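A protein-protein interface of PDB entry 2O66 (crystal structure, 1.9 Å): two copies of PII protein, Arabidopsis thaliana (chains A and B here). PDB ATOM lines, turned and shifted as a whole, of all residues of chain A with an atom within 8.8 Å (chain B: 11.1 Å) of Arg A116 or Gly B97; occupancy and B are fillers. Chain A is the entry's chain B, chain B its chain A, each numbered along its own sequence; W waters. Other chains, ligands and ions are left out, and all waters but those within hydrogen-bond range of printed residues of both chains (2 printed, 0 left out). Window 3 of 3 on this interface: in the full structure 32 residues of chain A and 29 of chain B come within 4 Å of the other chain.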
ATOM      1  N   ILE A 113     -27.041  17.233  15.138  1.00  0.00           N
ATOM      2  CA  ILE A 113     -25.597  17.068  14.978  1.00  0.00           C
ATOM      3  C   ILE A 113     -25.171  17.452  13.561  1.00  0.00           C
ATOM      4  O   ILE A 113     -25.799  17.032  12.587  1.00  0.00           O
ATOM      5  CB  ILE A 113     -25.137  15.602  15.285  1.00  0.00           C
ATOM      6  CG1 ILE A 113     -25.584  15.155  16.682  1.00  0.00           C
ATOM      7  CG2 ILE A 113     -23.629  15.464  15.166  1.00  0.00           C
ATOM      8  CD1 ILE A 113     -26.867  14.327  16.694  1.00  0.00           C
ATOM      9  N   ARG A 114     -24.118  18.257  13.448  1.00  0.00           N
ATOM     10  CA  ARG A 114     -23.519  18.563  12.144  1.00  0.00           C
ATOM     11  C   ARG A 114     -22.489  17.480  11.800  1.00  0.00           C
ATOM     12  O   ARG A 114     -21.517  17.286  12.537  1.00  0.00           O
ATOM     13  CB  ARG A 114     -22.867  19.957  12.164  1.00  0.00           C
ATOM     14  CG  ARG A 114     -22.287  20.420  10.821  1.00  0.00           C
ATOM     15  CD  ARG A 114     -21.669  21.830  10.905  1.00  0.00           C
ATOM     16  NE  ARG A 114     -22.483  22.771  11.687  1.00  0.00           N
ATOM     17  CZ  ARG A 114     -23.464  23.520  11.193  1.00  0.00           C
ATOM     18  NH1 ARG A 114     -23.771  23.459   9.910  1.00  0.00           N
ATOM     19  NH2 ARG A 114     -24.145  24.337  11.983  1.00  0.00           N
ATOM     20  N   VAL A 115     -22.710  16.774  10.692  1.00  0.00           N
ATOM     21  CA  VAL A 115     -21.849  15.645  10.297  1.00  0.00           C
ATOM     22  C   VAL A 115     -20.384  16.071  10.131  1.00  0.00           C
ATOM     23  O   VAL A 115     -19.480  15.406  10.632  1.00  0.00           O
ATOM     24  CB  VAL A 115     -22.360  14.939   9.000  1.00  0.00           C
ATOM     25  CG1 VAL A 115     -21.356  13.897   8.501  1.00  0.00           C
ATOM     26  CG2 VAL A 115     -23.715  14.278   9.233  1.00  0.00           C
ATOM     27  N   ARG A 116     -20.173  17.200   9.460  1.00  0.00           N
ATOM     28  CA  ARG A 116     -18.833  17.686   9.113  1.00  0.00           C
ATOM     29  C   ARG A 116     -17.915  17.942  10.318  1.00  0.00           C
ATOM     30  O   ARG A 116     -16.706  17.717  10.236  1.00  0.00           O
ATOM     31  CB  ARG A 116     -18.950  18.955   8.260  1.00  0.00           C
ATOM     32  CG  ARG A 116     -17.628  19.542   7.775  1.00  0.00           C
ATOM     33  CD  ARG A 116     -17.841  20.676   6.770  1.00  0.00           C
ATOM     34  NE  ARG A 116     -18.794  21.686   7.223  1.00  0.00           N
ATOM     35  CZ  ARG A 116     -18.484  22.749   7.963  1.00  0.00           C
ATOM     36  NH1 ARG A 116     -17.237  22.953   8.364  1.00  0.00           N
ATOM     37  NH2 ARG A 116     -19.429  23.614   8.308  1.00  0.00           N
ATOM     38  N   THR A 117     -18.494  18.401  11.427  1.00  0.00           N
ATOM     39  CA  THR A 117     -17.721  18.884  12.574  1.00  0.00           C
ATOM     40  C   THR A 117     -17.998  18.128  13.873  1.00  0.00           C
ATOM     41  O   THR A 117     -17.228  18.222  14.835  1.00  0.00           O
ATOM     42  CB  THR A 117     -18.000  20.377  12.830  1.00  0.00           C
ATOM     43  OG1 THR A 117     -19.394  20.556  13.104  1.00  0.00           O
ATOM     44  CG2 THR A 117     -17.617  21.225  11.625  1.00  0.00           C
ATOM     45  N   GLY A 118     -19.106  17.396  13.914  1.00  0.00           N
ATOM     46  CA  GLY A 118     -19.535  16.747  15.145  1.00  0.00           C
ATOM     47  C   GLY A 118     -20.160  17.725  16.129  1.00  0.00           C
ATOM     48  O   GLY A 118     -20.482  17.346  17.255  1.00  0.00           O
ATOM     49  N   GLU A 119     -20.332  18.981  15.705  1.00  0.00           N
ATOM     50  CA  GLU A 119     -21.004  19.993  16.522  1.00  0.00           C
ATOM     51  C   GLU A 119     -22.421  19.546  16.839  1.00  0.00           C
ATOM     52  O   GLU A 119     -23.085  18.925  16.009  1.00  0.00           O
ATOM     53  CB  GLU A 119     -21.044  21.345  15.823  1.00  0.00           C
ATOM     54  CG  GLU A 119     -19.731  22.107  15.858  1.00  0.00           C
ATOM     55  CD  GLU A 119     -19.738  23.297  14.921  1.00  0.00           C
ATOM     56  OE1 GLU A 119     -19.980  23.110  13.706  1.00  0.00           O
ATOM     57  OE2 GLU A 119     -19.499  24.424  15.402  1.00  0.00           O
ATOM     58  N   LYS A 123     -24.955  24.978  18.107  1.00  0.00           N
ATOM     59  CA  LYS A 123     -23.856  25.087  17.142  1.00  0.00           C
ATOM     60  C   LYS A 123     -24.092  24.268  15.867  1.00  0.00           C
ATOM     61  O   LYS A 123     -23.334  24.387  14.902  1.00  0.00           O
ATOM     62  CB  LYS A 123     -22.533  24.661  17.792  1.00  0.00           C
ATOM     63  CG  LYS A 123     -21.955  25.658  18.791  1.00  0.00           C
ATOM     64  CD  LYS A 123     -21.237  26.811  18.094  1.00  0.00           C
ATOM     65  CE  LYS A 123     -20.629  27.784  19.100  1.00  0.00           C
ATOM     66  NZ  LYS A 123     -19.447  27.205  19.802  1.00  0.00           N
ATOM     67  N   ALA A 124     -25.145  23.449  15.868  1.00  0.00           N
ATOM     68  CA  ALA A 124     -25.399  22.502  14.780  1.00  0.00           C
ATOM     69  C   ALA A 124     -26.683  22.765  13.990  1.00  0.00           C
ATOM     70  O   ALA A 124     -26.880  22.187  12.923  1.00  0.00           O
ATOM     71  CB  ALA A 124     -25.404  21.076  15.323  1.00  0.00           C
ATOM     72  N   LYS A 126     -28.090  25.660  12.556  1.00  0.00           N
ATOM     73  CA  LYS A 126     -28.100  26.555  11.396  1.00  0.00           C
ATOM     74  C   LYS A 126     -27.532  25.875  10.152  1.00  0.00           C
ATOM     75  O   LYS A 126     -26.569  25.110  10.236  1.00  0.00           O
ATOM     76  CB  LYS A 126     -27.356  27.866  11.695  1.00  0.00           C
ATOM     77  CG  LYS A 126     -27.993  28.735  12.799  1.00  0.00           C
ATOM     78  CD  LYS A 126     -29.431  29.149  12.465  1.00  0.00           C
ATOM     79  CE  LYS A 126     -30.004  30.157  13.474  1.00  0.00           C
ATOM     80  NZ  LYS A 126     -30.200  29.603  14.847  1.00  0.00           N
ATOM     81  N   MET A 127     -28.150  26.140   9.005  1.00  0.00           N
ATOM     82  CA  MET A 127     -27.674  25.596   7.735  1.00  0.00           C
ATOM     83  C   MET A 127     -26.486  26.414   7.238  1.00  0.00           C
ATOM     84  O   MET A 127     -26.561  27.640   7.147  1.00  0.00           O
ATOM     85  CB  MET A 127     -28.800  25.571   6.700  1.00  0.00           C
ATOM     86  CG  MET A 127     -29.842  24.485   6.949  1.00  0.00           C
ATOM     87  SD  MET A 127     -29.373  22.899   6.231  1.00  0.00           S
ATOM     88  CE  MET A 127     -30.711  21.842   6.791  1.00  0.00           C
ATOM     89  N   THR A 128     -25.384  25.728   6.941  1.00  0.00           N
ATOM     90  CA  THR A 128     -24.146  26.386   6.513  1.00  0.00           C
ATOM     91  C   THR A 128     -23.701  25.908   5.132  1.00  0.00           C
ATOM     92  O   THR A 128     -22.510  25.917   4.812  1.00  0.00           O
ATOM     93  CB  THR A 128     -22.997  26.178   7.532  1.00  0.00           C
ATOM     94  OG1 THR A 128     -22.748  24.777   7.703  1.00  0.00           O
ATOM     95  CG2 THR A 128     -23.339  26.804   8.880  1.00  0.00           C
ATOM     96  N   GLY A 129     -24.662  25.483   4.316  1.00  0.00           N
ATOM     97  CA  GLY A 129     -24.380  25.122   2.931  1.00  0.00           C
ATOM     98  C   GLY A 129     -24.298  26.376   2.078  1.00  0.00           C
ATOM     99  O   GLY A 129     -24.812  27.428   2.466  1.00  0.00           O
ATOM    100  N   ALA B  18     -30.534  10.777   9.413  1.00  0.00           N
ATOM    101  CA  ALA B  18     -29.338  11.404   8.854  1.00  0.00           C
ATOM    102  C   ALA B  18     -29.573  11.871   7.419  1.00  0.00           C
ATOM    103  O   ALA B  18     -29.939  11.077   6.556  1.00  0.00           O
ATOM    104  CB  ALA B  18     -28.165  10.443   8.909  1.00  0.00           C
ATOM    105  N   ILE B  19     -29.358  13.159   7.171  1.00  0.00           N
ATOM    106  CA  ILE B  19     -29.481  13.707   5.822  1.00  0.00           C
ATOM    107  C   ILE B  19     -28.068  13.908   5.314  1.00  0.00           C
ATOM    108  O   ILE B  19     -27.380  14.812   5.774  1.00  0.00           O
ATOM    109  CB  ILE B  19     -30.220  15.073   5.809  1.00  0.00           C
ATOM    110  CG1 ILE B  19     -31.469  15.050   6.697  1.00  0.00           C
ATOM    111  CG2 ILE B  19     -30.550  15.505   4.372  1.00  0.00           C
ATOM    112  CD1 ILE B  19     -32.557  14.129   6.236  1.00  0.00           C
ATOM    113  N   VAL B  20     -27.639  13.066   4.376  1.00  0.00           N
ATOM    114  CA  VAL B  20     -26.222  12.992   3.996  1.00  0.00           C
ATOM    115  C   VAL B  20     -26.053  12.937   2.476  1.00  0.00           C
ATOM    116  O   VAL B  20     -27.043  12.876   1.747  1.00  0.00           O
ATOM    117  CB  VAL B  20     -25.521  11.770   4.666  1.00  0.00           C
ATOM    118  CG1 VAL B  20     -25.623  11.853   6.196  1.00  0.00           C
ATOM    119  CG2 VAL B  20     -26.110  10.444   4.161  1.00  0.00           C
ATOM    120  N   ARG B  21     -24.805  12.970   2.006  1.00  0.00           N
ATOM    121  CA  ARG B  21     -24.508  12.904   0.568  1.00  0.00           C
ATOM    122  C   ARG B  21     -24.900  11.538  -0.008  1.00  0.00           C
ATOM    123  O   ARG B  21     -24.605  10.502   0.592  1.00  0.00           O
ATOM    124  CB  ARG B  21     -23.025  13.174   0.304  1.00  0.00           C
ATOM    125  CG  ARG B  21     -22.497  14.507   0.843  1.00  0.00           C
ATOM    126  CD  ARG B  21     -20.969  14.543   0.763  1.00  0.00           C
ATOM    127  NE  ARG B  21     -20.390  15.716   1.421  1.00  0.00           N
ATOM    128  CZ  ARG B  21     -20.203  16.899   0.834  1.00  0.00           C
ATOM    129  NH1 ARG B  21     -20.554  17.093  -0.435  1.00  0.00           N
ATOM    130  NH2 ARG B  21     -19.667  17.897   1.522  1.00  0.00           N
ATOM    131  N   TRP B  23     -23.790   9.624  -2.314  1.00  0.00           N
ATOM    132  CA  TRP B  23     -22.710   8.678  -2.600  1.00  0.00           C
ATOM    133  C   TRP B  23     -22.054   8.099  -1.341  1.00  0.00           C
ATOM    134  O   TRP B  23     -21.144   7.268  -1.438  1.00  0.00           O
ATOM    135  CB  TRP B  23     -21.669   9.291  -3.555  1.00  0.00           C
ATOM    136  CG  TRP B  23     -20.916  10.479  -3.009  1.00  0.00           C
ATOM    137  CD1 TRP B  23     -21.331  11.779  -3.002  1.00  0.00           C
ATOM    138  CD2 TRP B  23     -19.610  10.471  -2.415  1.00  0.00           C
ATOM    139  NE1 TRP B  23     -20.371  12.580  -2.430  1.00  0.00           N
ATOM    140  CE2 TRP B  23     -19.304  11.803  -2.061  1.00  0.00           C
ATOM    141  CE3 TRP B  23     -18.670   9.465  -2.146  1.00  0.00           C
ATOM    142  CZ2 TRP B  23     -18.098  12.159  -1.450  1.00  0.00           C
ATOM    143  CZ3 TRP B  23     -17.466   9.820  -1.540  1.00  0.00           C
ATOM    144  CH2 TRP B  23     -17.194  11.158  -1.198  1.00  0.00           C
ATOM    145  N   ARG B  24     -22.530   8.523  -0.167  1.00  0.00           N
ATOM    146  CA  ARG B  24     -22.035   7.993   1.110  1.00  0.00           C
ATOM    147  C   ARG B  24     -22.939   6.914   1.727  1.00  0.00           C
ATOM    148  O   ARG B  24     -22.616   6.378   2.793  1.00  0.00           O
ATOM    149  CB  ARG B  24     -21.789   9.121   2.128  1.00  0.00           C
ATOM    150  CG  ARG B  24     -20.813  10.206   1.680  1.00  0.00           C
ATOM    151  CD  ARG B  24     -19.419   9.664   1.403  1.00  0.00           C
ATOM    152  NE  ARG B  24     -18.708   9.282   2.618  1.00  0.00           N
ATOM    153  CZ  ARG B  24     -17.411   8.992   2.670  1.00  0.00           C
ATOM    154  NH1 ARG B  24     -16.666   9.042   1.573  1.00  0.00           N
ATOM    155  NH2 ARG B  24     -16.858   8.653   3.826  1.00  0.00           N
ATOM    156  N   LYS B  71     -29.759  14.976  -1.662  1.00  0.00           N
ATOM    157  CA  LYS B  71     -29.315  14.315  -0.443  1.00  0.00           C
ATOM    158  C   LYS B  71     -30.103  13.028  -0.286  1.00  0.00           C
ATOM    159  O   LYS B  71     -31.104  12.801  -0.984  1.00  0.00           O
ATOM    160  CB  LYS B  71     -29.558  15.202   0.788  1.00  0.00           C
ATOM    161  CG  LYS B  71     -28.698  16.466   0.906  1.00  0.00           C
ATOM    162  CD  LYS B  71     -27.284  16.155   1.388  1.00  0.00           C
ATOM    163  CE  LYS B  71     -26.758  17.221   2.354  1.00  0.00           C
ATOM    164  NZ  LYS B  71     -26.720  18.596   1.767  1.00  0.00           N
ATOM    165  N   ILE B  87     -24.896   7.510  16.118  1.00  0.00           N
ATOM    166  CA  ILE B  87     -24.435   8.852  15.719  1.00  0.00           C
ATOM    167  C   ILE B  87     -22.978   8.825  15.240  1.00  0.00           C
ATOM    168  O   ILE B  87     -22.674   9.296  14.139  1.00  0.00           O
ATOM    169  CB  ILE B  87     -24.601   9.901  16.857  1.00  0.00           C
ATOM    170  CG1 ILE B  87     -26.082  10.182  17.130  1.00  0.00           C
ATOM    171  CG2 ILE B  87     -23.868  11.201  16.511  1.00  0.00           C
ATOM    172  CD1 ILE B  87     -26.343  10.968  18.411  1.00  0.00           C
ATOM    173  N   ASN B  88     -22.089   8.255  16.055  1.00  0.00           N
ATOM    174  CA  ASN B  88     -20.656   8.240  15.744  1.00  0.00           C
ATOM    175  C   ASN B  88     -20.348   7.501  14.451  1.00  0.00           C
ATOM    176  O   ASN B  88     -19.509   7.933  13.651  1.00  0.00           O
ATOM    177  CB  ASN B  88     -19.848   7.635  16.902  1.00  0.00           C
ATOM    178  CG  ASN B  88     -19.630   8.615  18.054  1.00  0.00           C
ATOM    179  OD1 ASN B  88     -19.009   8.269  19.061  1.00  0.00           O
ATOM    180  ND2 ASN B  88     -20.131   9.837  17.911  1.00  0.00           N
ATOM    181  N   ILE B  90     -22.496   6.857  11.870  1.00  0.00           N
ATOM    182  CA  ILE B  90     -23.001   7.646  10.739  1.00  0.00           C
ATOM    183  C   ILE B  90     -22.003   8.740  10.340  1.00  0.00           C
ATOM    184  O   ILE B  90     -21.681   8.883   9.158  1.00  0.00           O
ATOM    185  CB  ILE B  90     -24.402   8.247  11.020  1.00  0.00           C
ATOM    186  CG1 ILE B  90     -25.448   7.130  11.074  1.00  0.00           C
ATOM    187  CG2 ILE B  90     -24.784   9.261   9.934  1.00  0.00           C
ATOM    188  CD1 ILE B  90     -26.811   7.567  11.616  1.00  0.00           C
ATOM    189  N   ILE B  91     -21.512   9.492  11.323  1.00  0.00           N
ATOM    190  CA  ILE B  91     -20.477  10.505  11.075  1.00  0.00           C
ATOM    191  C   ILE B  91     -19.253   9.887  10.384  1.00  0.00           C
ATOM    192  O   ILE B  91     -18.752  10.432   9.397  1.00  0.00           O
ATOM    193  CB  ILE B  91     -20.066  11.253  12.373  1.00  0.00           C
ATOM    194  CG1 ILE B  91     -21.226  12.118  12.885  1.00  0.00           C
ATOM    195  CG2 ILE B  91     -18.820  12.122  12.134  1.00  0.00           C
ATOM    196  CD1 ILE B  91     -20.986  12.764  14.252  1.00  0.00           C
ATOM    197  N   GLU B  92     -18.796   8.740  10.889  1.00  0.00           N
ATOM    198  CA  GLU B  92     -17.652   8.027  10.305  1.00  0.00           C
ATOM    199  C   GLU B  92     -17.898   7.684   8.831  1.00  0.00           C
ATOM    200  O   GLU B  92     -17.015   7.865   7.985  1.00  0.00           O
ATOM    201  CB  GLU B  92     -17.339   6.762  11.121  1.00  0.00           C
ATOM    202  CG  GLU B  92     -16.102   5.983  10.667  1.00  0.00           C
ATOM    203  CD  GLU B  92     -15.810   4.768  11.540  1.00  0.00           C
ATOM    204  OE1 GLU B  92     -16.249   4.742  12.710  1.00  0.00           O
ATOM    205  OE2 GLU B  92     -15.135   3.838  11.050  1.00  0.00           O
ATOM    206  N   GLY B  93     -19.103   7.212   8.528  1.00  0.00           N
ATOM    207  CA  GLY B  93     -19.466   6.839   7.167  1.00  0.00           C
ATOM    208  C   GLY B  93     -19.723   8.011   6.238  1.00  0.00           C
ATOM    209  O   GLY B  93     -19.434   7.927   5.043  1.00  0.00           O
ATOM    210  N   ALA B  94     -20.250   9.109   6.784  1.00  0.00           N
ATOM    211  CA  ALA B  94     -20.781  10.202   5.964  1.00  0.00           C
ATOM    212  C   ALA B  94     -19.870  11.427   5.814  1.00  0.00           C
ATOM    213  O   ALA B  94     -20.003  12.180   4.847  1.00  0.00           O
ATOM    214  CB  ALA B  94     -22.147  10.627   6.483  1.00  0.00           C
ATOM    215  N   ARG B  95     -18.963  11.630   6.767  1.00  0.00           N
ATOM    216  CA  ARG B  95     -18.104  12.816   6.781  1.00  0.00           C
ATOM    217  C   ARG B  95     -17.051  12.810   5.665  1.00  0.00           C
ATOM    218  O   ARG B  95     -16.395  11.793   5.423  1.00  0.00           O
ATOM    219  CB  ARG B  95     -17.439  12.974   8.150  1.00  0.00           C
ATOM    220  CG  ARG B  95     -16.398  14.086   8.236  1.00  0.00           C
ATOM    221  CD  ARG B  95     -16.534  14.838   9.539  1.00  0.00           C
ATOM    222  NE  ARG B  95     -15.800  14.238  10.643  1.00  0.00           N
ATOM    223  CZ  ARG B  95     -16.085  14.426  11.932  1.00  0.00           C
ATOM    224  NH1 ARG B  95     -17.116  15.178  12.303  1.00  0.00           N
ATOM    225  NH2 ARG B  95     -15.342  13.837  12.857  1.00  0.00           N
ATOM    226  N   THR B  96     -16.915  13.957   4.997  1.00  0.00           N
ATOM    227  CA  THR B  96     -15.852  14.199   4.016  1.00  0.00           C
ATOM    228  C   THR B  96     -14.976  15.381   4.441  1.00  0.00           C
ATOM    229  O   THR B  96     -13.837  15.508   3.988  1.00  0.00           O
ATOM    230  CB  THR B  96     -16.406  14.528   2.611  1.00  0.00           C
ATOM    231  OG1 THR B  96     -17.063  15.807   2.642  1.00  0.00           O
ATOM    232  CG2 THR B  96     -17.369  13.450   2.114  1.00  0.00           C
ATOM    233  N   GLY B  97     -15.524  16.250   5.290  1.00  0.00           N
ATOM    234  CA  GLY B  97     -14.813  17.434   5.774  1.00  0.00           C
ATOM    235  C   GLY B  97     -15.161  18.693   5.002  1.00  0.00           C
ATOM    236  O   GLY B  97     -14.877  19.806   5.446  1.00  0.00           O
ATOM    237  N   GLU B  98     -15.775  18.515   3.838  1.00  0.00           N
ATOM    238  CA  GLU B  98     -16.189  19.637   3.008  1.00  0.00           C
ATOM    239  C   GLU B  98     -17.604  20.074   3.375  1.00  0.00           C
ATOM    240  O   GLU B  98     -18.411  19.262   3.839  1.00  0.00           O
ATOM    241  CB  GLU B  98     -16.130  19.255   1.528  1.00  0.00           C
ATOM    242  CG  GLU B  98     -14.748  18.827   1.051  1.00  0.00           C
ATOM    243  CD  GLU B  98     -14.682  18.604  -0.450  1.00  0.00           C
ATOM    244  OE1 GLU B  98     -15.745  18.575  -1.108  1.00  0.00           O
ATOM    245  OE2 GLU B  98     -13.557  18.451  -0.975  1.00  0.00           O
ATOM    246  N   ILE B  99     -17.886  21.363   3.177  1.00  0.00           N
ATOM    247  CA  ILE B  99     -19.230  21.911   3.323  1.00  0.00           C
ATOM    248  C   ILE B  99     -20.212  21.038   2.541  1.00  0.00           C
ATOM    249  O   ILE B  99     -19.985  20.742   1.361  1.00  0.00           O
ATOM    250  CB  ILE B  99     -19.314  23.369   2.785  1.00  0.00           C
ATOM    251  CG1 ILE B  99     -18.448  24.332   3.618  1.00  0.00           C
ATOM    252  CG2 ILE B  99     -20.767  23.835   2.683  1.00  0.00           C
ATOM    253  CD1 ILE B  99     -19.058  24.804   4.934  1.00  0.00           C
ATOM    254  N   GLY B 100     -21.286  20.620   3.209  1.00  0.00           N
ATOM    255  CA  GLY B 100     -22.341  19.838   2.569  1.00  0.00           C
ATOM    256  C   GLY B 100     -22.463  18.396   3.042  1.00  0.00           C
ATOM    257  O   GLY B 100     -23.130  17.588   2.387  1.00  0.00           O
ATOM    258  N   ASP B 101     -21.827  18.068   4.167  1.00  0.00           N
ATOM    259  CA  ASP B 101     -21.871  16.700   4.713  1.00  0.00           C
ATOM    260  C   ASP B 101     -23.238  16.321   5.308  1.00  0.00           C
ATOM    261  O   ASP B 101     -23.534  15.131   5.489  1.00  0.00           O
ATOM    262  CB  ASP B 101     -20.785  16.495   5.777  1.00  0.00           C
ATOM    263  CG  ASP B 101     -19.404  16.244   5.187  1.00  0.00           C
ATOM    264  OD1 ASP B 101     -19.278  16.028   3.962  1.00  0.00           O
ATOM    265  OD2 ASP B 101     -18.437  16.232   5.976  1.00  0.00           O
ATOM    266  N   GLY B 102     -24.053  17.325   5.631  1.00  0.00           N
ATOM    267  CA  GLY B 102     -25.415  17.082   6.120  1.00  0.00           C
ATOM    268  C   GLY B 102     -25.542  17.133   7.632  1.00  0.00           C
ATOM    269  O   GLY B 102     -24.617  17.549   8.329  1.00  0.00           O
ATOM    270  N   LYS B 103     -26.698  16.707   8.134  1.00  0.00           N
ATOM    271  CA  LYS B 103     -27.009  16.776   9.563  1.00  0.00           C
ATOM    272  C   LYS B 103     -27.628  15.472  10.050  1.00  0.00           C
ATOM    273  O   LYS B 103     -28.168  14.699   9.257  1.00  0.00           O
ATOM    274  CB  LYS B 103     -27.995  17.915   9.848  1.00  0.00           C
ATOM    275  CG  LYS B 103     -27.470  19.322   9.607  1.00  0.00           C
ATOM    276  CD  LYS B 103     -28.511  20.364  10.016  1.00  0.00           C
ATOM    277  CE  LYS B 103     -28.121  21.771   9.575  1.00  0.00           C
ATOM    278  NZ  LYS B 103     -26.914  22.277  10.282  1.00  0.00           N
ATOM    279  N   ILE B 104     -27.562  15.248  11.359  1.00  0.00           N
ATOM    280  CA  ILE B 104     -28.256  14.124  11.996  1.00  0.00           C
ATOM    281  C   ILE B 104     -29.267  14.675  12.994  1.00  0.00           C
ATOM    282  O   ILE B 104     -28.940  15.559  13.788  1.00  0.00           O
ATOM    283  CB  ILE B 104     -27.269  13.184  12.735  1.00  0.00           C
ATOM    284  CG1 ILE B 104     -26.283  12.554  11.744  1.00  0.00           C
ATOM    285  CG2 ILE B 104     -28.031  12.112  13.525  1.00  0.00           C
ATOM    286  CD1 ILE B 104     -24.986  12.071  12.383  1.00  0.00           C
HETATM  287  O   HOH W   1     -22.173  18.707   7.891  1.00  0.00           O
HETATM  288  O   HOH W   2     -14.771  21.334   8.401  1.00  0.00           O
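The guanidinium group (NH1) of Arg A114 sits close to the side-chain amino group (NZ) of Lys B103. The backbone carbonyl oxygen (O) of Gly B102 lies within hydrogen-bond range of the backbone NH (N) of Val A115 (3.1 Å). The guanidinium group of Arg B95 is in hydrogen-bond range of the backbone carbonyl oxygen of Val A115. The side-chain amino group (NZ) of Lys B103 is in hydrogen-bond range of the backbone carbonyl oxygen (O) of Lys A126 (2.9 Å). N of Gly A118 lies close to NH1 of Arg B95 (3.4 Å). NH1 of Arg B95 lies close to O of Arg A116 (3.3 Å). The backbone NH (N) of Ile B104 sits at hydrogen-bond distance from the backbone carbonyl oxygen (O) of Ile A113 (2.8 Å). O of Ala A124 is in hydrogen-bond range of NZ of Lys B103 (2.6 Å).
The guanidinium group (NH2) of Arg B21 sits at hydrogen-bond distance from the backbone carbonyl oxygen (O) of Glu B98 (3.0 Å). N of Glu B98 sits at hydrogen-bond distance from OG1 of Thr B96, 3.2 Å away. NH2 of Arg B21 lies within hydrogen-bond range of O of Ile B99, at 2.9 Å. The guanidinium group of Arg B21 lies within salt-bridge range of the side-chain carboxylate of Asp B101 (2.8 Å). The side-chain carboxylate (OE1) of Glu A119 is in hydrogen-bond range of the side-chain hydroxyl (OG1) of Thr A117, at 2.7 Å. NH2 of Arg A114 sits at hydrogen-bond distance from O of Lys A123.
Among the printed residues, pairs that only touch across the chains: Ile A113 with Lys B103, Arg A116 with Glu B98, Arg A116 with Gly B97, Thr A128 with Ile B99, Thr A117 with Arg B95, Arg A116 with Asp B101, Arg A116 with Ile B99, Val A115 with Ile B91, Val A115 with Asp B101, Met A127 with Lys B103, Ile A113 with Ile B87, Gly A129 with Ile B99, Ile A113 with Ile B91, Val A115 with Ala B94 and Val A115 with Ile B104.
Arg A116 touches five residues of chain B. Gly B97 touches just one residue of chain A: Arg A116 (3.4 Å). Arg A114 touches just one residue of chain B: Lys B103. Thr A117 touches just one residue of chain B: Arg B95 (3.5 Å). Of chain B, only Ile B99 (3.5 Å) comes within 4 Å of Thr A128. No residue of chain A comes within 4 Å of Thr B96. Of the printed residues of chain A, Ile B87 touches Ile A113. Of the printed residues of chain A, Arg B95 touches Val A115, Arg A116, Thr A117 and Gly A118. Printed residues of chain A within 4 Å of Ile B99: Arg A116 (3.6 Å), Thr A128 (3.5 Å) and Gly A129 (3.8 Å). The nearest residue of chain B that does not touch Arg A116 is Gly B102 (4.6 Å). The nearest residue of chain A that does not touch Gly B97 is Val A115 (6.7 Å).
Hydrophobic or aromatic side chains of chain B that line the printed part of chain A: Ile B87, Ile B91, Ala B94, Ile B99 and Ile B104. Along chain B the printed residues that touch a printed residue of chain A span positions 87 to 104. Of the 13 printed residues of chain A, 11 touch a printed residue of chain B. Printed residues of chain A that touch a printed residue of chain B: Ile A113, Arg A114, Val A115, Arg A116, Thr A117, Gly A118, Ala A124, Lys A126, Met A127, Thr A128 and Gly A129. Among the printed residues, 23 pairs touch across the chains. Among the printed residues, no Asp or Glu carboxylate lies within 4 Å of a Lys or Arg side-chain nitrogen of the other chain.
No position is printed for both chains. Of the 23 pairs that touch across the chains among the printed residues, none has its exchanged pair printed and touching as well.
Water W1 lies within hydrogen-bond range of the backbone carbonyl oxygen of Gly B102 (2.7 Å), the backbone NH of Arg A116 (3.0 Å) and the backbone NH of Val A115 (3.4 Å). Water W2 lies within hydrogen-bond range of NH1 of Arg A116 (3.0 Å) and O of Gly B97 (3.3 Å).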
